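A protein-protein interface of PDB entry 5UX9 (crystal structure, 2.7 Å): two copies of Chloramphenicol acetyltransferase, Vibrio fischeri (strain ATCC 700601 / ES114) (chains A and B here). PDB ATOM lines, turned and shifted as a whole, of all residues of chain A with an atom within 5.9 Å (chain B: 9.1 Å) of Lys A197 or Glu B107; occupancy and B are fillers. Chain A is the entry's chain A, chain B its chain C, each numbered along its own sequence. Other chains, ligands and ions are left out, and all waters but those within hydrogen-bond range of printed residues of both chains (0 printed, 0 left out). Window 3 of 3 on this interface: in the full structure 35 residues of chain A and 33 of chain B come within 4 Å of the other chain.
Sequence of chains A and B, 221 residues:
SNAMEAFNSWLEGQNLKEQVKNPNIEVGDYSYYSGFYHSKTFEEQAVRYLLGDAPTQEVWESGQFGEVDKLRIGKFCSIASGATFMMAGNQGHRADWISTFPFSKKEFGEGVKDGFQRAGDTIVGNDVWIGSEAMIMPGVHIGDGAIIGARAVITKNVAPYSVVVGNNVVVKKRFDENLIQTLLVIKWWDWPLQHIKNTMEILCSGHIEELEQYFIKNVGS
The side-chain hydroxyl of Tyr A30 is in hydrogen-bond range of the side-chain carboxylate of Glu B107 (3.5 Å).
No position is printed for both chains.
Of the 11 pairs that touch across the chains among the printed residues, none has its exchanged pair printed and touching as well.
Phe B101 touches Tyr A30 (CZ to O, 3.2 Å).
Phe B108 touches Tyr A30.
Phe B108 touches Leu A193.
Lys A197 touches Glu B107 (CE to O, 3.2 Å).
Lys A197 touches Phe B108.
Phe B103 touches Met A200.
CB of Phe B108 touches CE of Met A200 (3.6 Å).
Met A200 touches Gly B111 (CG to O, 3.4 Å).
CG2 of Val B112 touches CG of Met A200, at 3.6 Å.
O of Gly B111 touches N of Glu A201, 3.7 Å away.
Printed residues of chain B within 4 Å of Leu A193: Phe B108.
Of chain B, only Glu B107 (3.2 Å) and Phe B108 (3.9 Å) come within 4 Å of Lys A197.
No residue of chain B comes within 4 Å of Asn A198.
Of the printed residues of chain B, Glu A201 touches Gly B111 (3.7 Å).
Printed residues of chain A within 4 Å of Glu B107: Tyr A30 and Lys A197.
The nearest residue of chain A that does not touch Glu B107 is Leu A193 (4.7 Å).
Of the 11 printed residues of chain A, 5 touch a printed residue of chain B.
Printed residues of chain A that touch a printed residue of chain B: Tyr A30, Leu A193, Lys A197, Met A200 and Glu A201.
Hydrophobic or aromatic side chains of chain A that line the printed part of chain B: Tyr A30, Leu A193 and Met A200.
Among the printed residues, no Asp or Glu carboxylate lies within 4 Å of a Lys or Arg side-chain nitrogen of the other chain.
OG of Ser B104 sits at hydrogen-bond distance from N of Glu B107, 3.2 Å away.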
ATOM      1  N   TYR A  30     -24.366  -7.359   0.872  1.00  0.00           N
ATOM      2  CA  TYR A  30     -23.805  -7.733  -0.425  1.00  0.00           C
ATOM      3  C   TYR A  30     -24.853  -7.880  -1.527  1.00  0.00           C
ATOM      4  O   TYR A  30     -24.498  -7.993  -2.704  1.00  0.00           O
ATOM      5  CB  TYR A  30     -22.989  -9.026  -0.297  1.00  0.00           C
ATOM      6  CG  TYR A  30     -21.764  -8.885   0.581  1.00  0.00           C
ATOM      7  CD1 TYR A  30     -20.657  -8.165   0.154  1.00  0.00           C
ATOM      8  CD2 TYR A  30     -21.718  -9.472   1.840  1.00  0.00           C
ATOM      9  CE1 TYR A  30     -19.536  -8.032   0.955  1.00  0.00           C
ATOM     10  CE2 TYR A  30     -20.602  -9.344   2.647  1.00  0.00           C
ATOM     11  CZ  TYR A  30     -19.515  -8.624   2.201  1.00  0.00           C
ATOM     12  OH  TYR A  30     -18.403  -8.496   3.004  1.00  0.00           O
ATOM     13  N   PRO A 192     -18.985 -15.842   9.207  1.00  0.00           N
ATOM     14  CA  PRO A 192     -18.040 -14.719   9.184  1.00  0.00           C
ATOM     15  C   PRO A 192     -17.390 -14.617   7.811  1.00  0.00           C
ATOM     16  O   PRO A 192     -17.108 -15.628   7.163  1.00  0.00           O
ATOM     17  CB  PRO A 192     -17.024 -15.085  10.271  1.00  0.00           C
ATOM     18  CG  PRO A 192     -17.775 -15.990  11.199  1.00  0.00           C
ATOM     19  CD  PRO A 192     -18.731 -16.762  10.331  1.00  0.00           C
ATOM     20  N   LEU A 193     -17.158 -13.376   7.368  1.00  0.00           N
ATOM     21  CA  LEU A 193     -16.682 -13.141   6.006  1.00  0.00           C
ATOM     22  C   LEU A 193     -15.361 -13.849   5.734  1.00  0.00           C
ATOM     23  O   LEU A 193     -15.080 -14.224   4.591  1.00  0.00           O
ATOM     24  CB  LEU A 193     -16.544 -11.640   5.755  1.00  0.00           C
ATOM     25  CG  LEU A 193     -15.706 -11.208   4.550  1.00  0.00           C
ATOM     26  CD1 LEU A 193     -16.546 -11.335   3.298  1.00  0.00           C
ATOM     27  CD2 LEU A 193     -15.178  -9.788   4.697  1.00  0.00           C
ATOM     28  N   GLN A 194     -14.548 -14.059   6.769  1.00  0.00           N
ATOM     29  CA  GLN A 194     -13.293 -14.783   6.595  1.00  0.00           C
ATOM     30  C   GLN A 194     -13.546 -16.206   6.113  1.00  0.00           C
ATOM     31  O   GLN A 194     -12.895 -16.678   5.173  1.00  0.00           O
ATOM     32  CB  GLN A 194     -12.508 -14.784   7.908  1.00  0.00           C
ATOM     33  N   HIS A 195     -14.497 -16.902   6.741  1.00  0.00           N
ATOM     34  CA  HIS A 195     -14.792 -18.275   6.343  1.00  0.00           C
ATOM     35  C   HIS A 195     -15.344 -18.333   4.925  1.00  0.00           C
ATOM     36  O   HIS A 195     -15.062 -19.277   4.177  1.00  0.00           O
ATOM     37  CB  HIS A 195     -15.773 -18.906   7.329  1.00  0.00           C
ATOM     38  CG  HIS A 195     -15.150 -19.299   8.632  1.00  0.00           C
ATOM     39  ND1 HIS A 195     -13.889 -19.850   8.716  1.00  0.00           N
ATOM     40  CD2 HIS A 195     -15.614 -19.225   9.901  1.00  0.00           C
ATOM     41  CE1 HIS A 195     -13.603 -20.097   9.982  1.00  0.00           C
ATOM     42  NE2 HIS A 195     -14.633 -19.728  10.721  1.00  0.00           N
ATOM     43  N   ILE A 196     -16.138 -17.332   4.537  1.00  0.00           N
ATOM     44  CA  ILE A 196     -16.606 -17.246   3.157  1.00  0.00           C
ATOM     45  C   ILE A 196     -15.426 -17.068   2.211  1.00  0.00           C
ATOM     46  O   ILE A 196     -15.364 -17.691   1.144  1.00  0.00           O
ATOM     47  CB  ILE A 196     -17.631 -16.103   3.013  1.00  0.00           C
ATOM     48  CG1 ILE A 196     -18.922 -16.448   3.754  1.00  0.00           C
ATOM     49  CG2 ILE A 196     -17.921 -15.815   1.549  1.00  0.00           C
ATOM     50  CD1 ILE A 196     -19.891 -15.291   3.851  1.00  0.00           C
ATOM     51  N   LYS A 197     -14.464 -16.224   2.598  1.00  0.00           N
ATOM     52  CA  LYS A 197     -13.275 -16.009   1.781  1.00  0.00           C
ATOM     53  C   LYS A 197     -12.490 -17.301   1.590  1.00  0.00           C
ATOM     54  O   LYS A 197     -12.023 -17.594   0.483  1.00  0.00           O
ATOM     55  CB  LYS A 197     -12.384 -14.943   2.421  1.00  0.00           C
ATOM     56  CG  LYS A 197     -12.804 -13.504   2.165  1.00  0.00           C
ATOM     57  CD  LYS A 197     -11.821 -12.534   2.813  1.00  0.00           C
ATOM     58  CE  LYS A 197     -12.161 -11.087   2.498  1.00  0.00           C
ATOM     59  N   ASN A 198     -12.331 -18.084   2.660  1.00  0.00           N
ATOM     60  CA  ASN A 198     -11.547 -19.313   2.561  1.00  0.00           C
ATOM     61  C   ASN A 198     -12.234 -20.345   1.674  1.00  0.00           C
ATOM     62  O   ASN A 198     -11.567 -21.075   0.932  1.00  0.00           O
ATOM     63  CB  ASN A 198     -11.296 -19.888   3.955  1.00  0.00           C
ATOM     64  CG  ASN A 198     -10.566 -18.919   4.863  1.00  0.00           C
ATOM     65  OD1 ASN A 198     -10.963 -18.706   6.008  1.00  0.00           O
ATOM     66  ND2 ASN A 198      -9.493 -18.324   4.353  1.00  0.00           N
ATOM     67  N   THR A 199     -13.563 -20.419   1.732  1.00  0.00           N
ATOM     68  CA  THR A 199     -14.443 -21.348   1.039  1.00  0.00           C
ATOM     69  C   THR A 199     -14.721 -20.941  -0.401  1.00  0.00           C
ATOM     70  O   THR A 199     -15.664 -21.461  -1.010  1.00  0.00           O
ATOM     71  CB  THR A 199     -15.765 -21.487   1.795  1.00  0.00           C
ATOM     72  OG1 THR A 199     -16.318 -20.187   2.034  1.00  0.00           O
ATOM     73  CG2 THR A 199     -15.541 -22.185   3.114  1.00  0.00           C
ATOM     74  N   MET A 200     -14.095 -19.882  -0.901  1.00  0.00           N
ATOM     75  CA  MET A 200     -14.458 -19.316  -2.194  1.00  0.00           C
ATOM     76  C   MET A 200     -14.260 -20.319  -3.330  1.00  0.00           C
ATOM     77  O   MET A 200     -15.044 -20.355  -4.278  1.00  0.00           O
ATOM     78  CB  MET A 200     -13.648 -18.048  -2.458  1.00  0.00           C
ATOM     79  CG  MET A 200     -14.199 -17.190  -3.578  1.00  0.00           C
ATOM     80  SD  MET A 200     -16.094 -16.785  -3.379  1.00  0.00           S
ATOM     81  CE  MET A 200     -16.070 -16.068  -1.569  1.00  0.00           C
ATOM     82  N   GLU A 201     -13.210 -21.137  -3.225  1.00  0.00           N
ATOM     83  CA  GLU A 201     -12.980 -22.169  -4.230  1.00  0.00           C
ATOM     84  C   GLU A 201     -14.085 -23.218  -4.218  1.00  0.00           C
ATOM     85  O   GLU A 201     -14.378 -23.821  -5.257  1.00  0.00           O
ATOM     86  CB  GLU A 201     -11.618 -22.829  -4.004  1.00  0.00           C
ATOM     87  CG  GLU A 201     -11.171 -23.741  -5.137  1.00  0.00           C
ATOM     88  N   PHE B 101     -24.235 -15.947  -6.884  1.00  0.00           N
ATOM     89  CA  PHE B 101     -23.806 -14.567  -6.712  1.00  0.00           C
ATOM     90  C   PHE B 101     -22.439 -14.364  -7.353  1.00  0.00           C
ATOM     91  O   PHE B 101     -21.528 -15.169  -7.128  1.00  0.00           O
ATOM     92  CB  PHE B 101     -23.751 -14.201  -5.234  1.00  0.00           C
ATOM     93  CG  PHE B 101     -23.459 -12.753  -4.981  1.00  0.00           C
ATOM     94  CD1 PHE B 101     -22.156 -12.311  -4.824  1.00  0.00           C
ATOM     95  CD2 PHE B 101     -24.488 -11.830  -4.906  1.00  0.00           C
ATOM     96  CE1 PHE B 101     -21.885 -10.977  -4.595  1.00  0.00           C
ATOM     97  CE2 PHE B 101     -24.224 -10.495  -4.676  1.00  0.00           C
ATOM     98  CZ  PHE B 101     -22.920 -10.067  -4.521  1.00  0.00           C
ATOM     99  N   PRO B 102     -22.257 -13.316  -8.152  1.00  0.00           N
ATOM    100  CA  PRO B 102     -20.946 -13.074  -8.768  1.00  0.00           C
ATOM    101  C   PRO B 102     -19.987 -12.364  -7.826  1.00  0.00           C
ATOM    102  O   PRO B 102     -19.892 -11.133  -7.833  1.00  0.00           O
ATOM    103  CB  PRO B 102     -21.291 -12.212  -9.987  1.00  0.00           C
ATOM    104  CG  PRO B 102     -22.527 -11.480  -9.580  1.00  0.00           C
ATOM    105  CD  PRO B 102     -23.278 -12.358  -8.613  1.00  0.00           C
ATOM    106  N   PHE B 103     -19.275 -13.139  -7.009  1.00  0.00           N
ATOM    107  CA  PHE B 103     -18.318 -12.565  -6.074  1.00  0.00           C
ATOM    108  C   PHE B 103     -17.212 -11.832  -6.826  1.00  0.00           C
ATOM    109  O   PHE B 103     -16.765 -12.272  -7.889  1.00  0.00           O
ATOM    110  CB  PHE B 103     -17.717 -13.659  -5.188  1.00  0.00           C
ATOM    111  CG  PHE B 103     -18.740 -14.494  -4.468  1.00  0.00           C
ATOM    112  CD1 PHE B 103     -19.218 -14.110  -3.224  1.00  0.00           C
ATOM    113  CD2 PHE B 103     -19.219 -15.668  -5.031  1.00  0.00           C
ATOM    114  CE1 PHE B 103     -20.159 -14.878  -2.559  1.00  0.00           C
ATOM    115  CE2 PHE B 103     -20.161 -16.440  -4.371  1.00  0.00           C
ATOM    116  CZ  PHE B 103     -20.630 -16.045  -3.134  1.00  0.00           C
ATOM    117  N   SER B 104     -16.779 -10.703  -6.273  1.00  0.00           N
ATOM    118  CA  SER B 104     -15.705  -9.917  -6.862  1.00  0.00           C
ATOM    119  C   SER B 104     -14.372 -10.294  -6.231  1.00  0.00           C
ATOM    120  O   SER B 104     -14.298 -10.580  -5.032  1.00  0.00           O
ATOM    121  CB  SER B 104     -15.960  -8.421  -6.679  1.00  0.00           C
ATOM    122  OG  SER B 104     -15.447  -7.967  -5.438  1.00  0.00           O
ATOM    123  N   LYS B 105     -13.316 -10.286  -7.048  1.00  0.00           N
ATOM    124  CA  LYS B 105     -11.994 -10.658  -6.552  1.00  0.00           C
ATOM    125  C   LYS B 105     -11.494  -9.685  -5.494  1.00  0.00           C
ATOM    126  O   LYS B 105     -10.806 -10.096  -4.551  1.00  0.00           O
ATOM    127  CB  LYS B 105     -11.001 -10.736  -7.712  1.00  0.00           C
ATOM    128  N   LYS B 106     -11.829  -8.399  -5.622  1.00  0.00           N
ATOM    129  CA  LYS B 106     -11.337  -7.412  -4.667  1.00  0.00           C
ATOM    130  C   LYS B 106     -11.929  -7.619  -3.278  1.00  0.00           C
ATOM    131  O   LYS B 106     -11.270  -7.320  -2.275  1.00  0.00           O
ATOM    132  CB  LYS B 106     -11.642  -6.000  -5.167  1.00  0.00           C
ATOM    133  N   GLU B 107     -13.153  -8.136  -3.196  1.00  0.00           N
ATOM    134  CA  GLU B 107     -13.839  -8.262  -1.917  1.00  0.00           C
ATOM    135  C   GLU B 107     -13.647  -9.624  -1.263  1.00  0.00           C
ATOM    136  O   GLU B 107     -13.639  -9.711  -0.029  1.00  0.00           O
ATOM    137  CB  GLU B 107     -15.336  -7.991  -2.099  1.00  0.00           C
ATOM    138  CG  GLU B 107     -16.125  -7.915  -0.802  1.00  0.00           C
ATOM    139  CD  GLU B 107     -15.865  -6.635  -0.033  1.00  0.00           C
ATOM    140  OE1 GLU B 107     -15.475  -5.630  -0.663  1.00  0.00           O
ATOM    141  OE2 GLU B 107     -16.051  -6.637   1.203  1.00  0.00           O
ATOM    142  N   PHE B 108     -13.481 -10.687  -2.051  1.00  0.00           N
ATOM    143  CA  PHE B 108     -13.483 -12.044  -1.516  1.00  0.00           C
ATOM    144  C   PHE B 108     -12.200 -12.816  -1.812  1.00  0.00           C
ATOM    145  O   PHE B 108     -12.176 -14.040  -1.634  1.00  0.00           O
ATOM    146  CB  PHE B 108     -14.696 -12.812  -2.048  1.00  0.00           C
ATOM    147  CG  PHE B 108     -16.015 -12.225  -1.624  1.00  0.00           C
ATOM    148  CD1 PHE B 108     -16.676 -11.316  -2.434  1.00  0.00           C
ATOM    149  CD2 PHE B 108     -16.590 -12.578  -0.413  1.00  0.00           C
ATOM    150  CE1 PHE B 108     -17.888 -10.772  -2.046  1.00  0.00           C
ATOM    151  CE2 PHE B 108     -17.803 -12.037  -0.019  1.00  0.00           C
ATOM    152  CZ  PHE B 108     -18.452 -11.134  -0.837  1.00  0.00           C
ATOM    153  N   GLY B 109     -11.139 -12.146  -2.254  1.00  0.00           N
ATOM    154  CA  GLY B 109      -9.848 -12.790  -2.393  1.00  0.00           C
ATOM    155  C   GLY B 109      -9.621 -13.418  -3.752  1.00  0.00           C
ATOM    156  O   GLY B 109     -10.488 -13.451  -4.629  1.00  0.00           O
ATOM    157  N   GLU B 110      -8.402 -13.938  -3.922  1.00  0.00           N
ATOM    158  CA  GLU B 110      -7.996 -14.527  -5.192  1.00  0.00           C
ATOM    159  C   GLU B 110      -8.669 -15.865  -5.470  1.00  0.00           C
ATOM    160  O   GLU B 110      -8.617 -16.336  -6.612  1.00  0.00           O
ATOM    161  CB  GLU B 110      -6.475 -14.696  -5.230  1.00  0.00           C
ATOM    162  N   GLY B 111      -9.298 -16.482  -4.471  1.00  0.00           N
ATOM    163  CA  GLY B 111      -9.977 -17.747  -4.675  1.00  0.00           C
ATOM    164  C   GLY B 111     -11.256 -17.672  -5.481  1.00  0.00           C
ATOM    165  O   GLY B 111     -11.930 -18.695  -5.634  1.00  0.00           O
ATOM    166  N   VAL B 112     -11.609 -16.499  -5.998  1.00  0.00           N
ATOM    167  CA  VAL B 112     -12.830 -16.341  -6.780  1.00  0.00           C
ATOM    168  C   VAL B 112     -12.623 -16.945  -8.161  1.00  0.00           C
ATOM    169  O   VAL B 112     -11.670 -16.599  -8.869  1.00  0.00           O
ATOM    170  CB  VAL B 112     -13.224 -14.859  -6.883  1.00  0.00           C
ATOM    171  CG1 VAL B 112     -14.446 -14.700  -7.774  1.00  0.00           C
ATOM    172  CG2 VAL B 112     -13.482 -14.275  -5.504  1.00  0.00           C
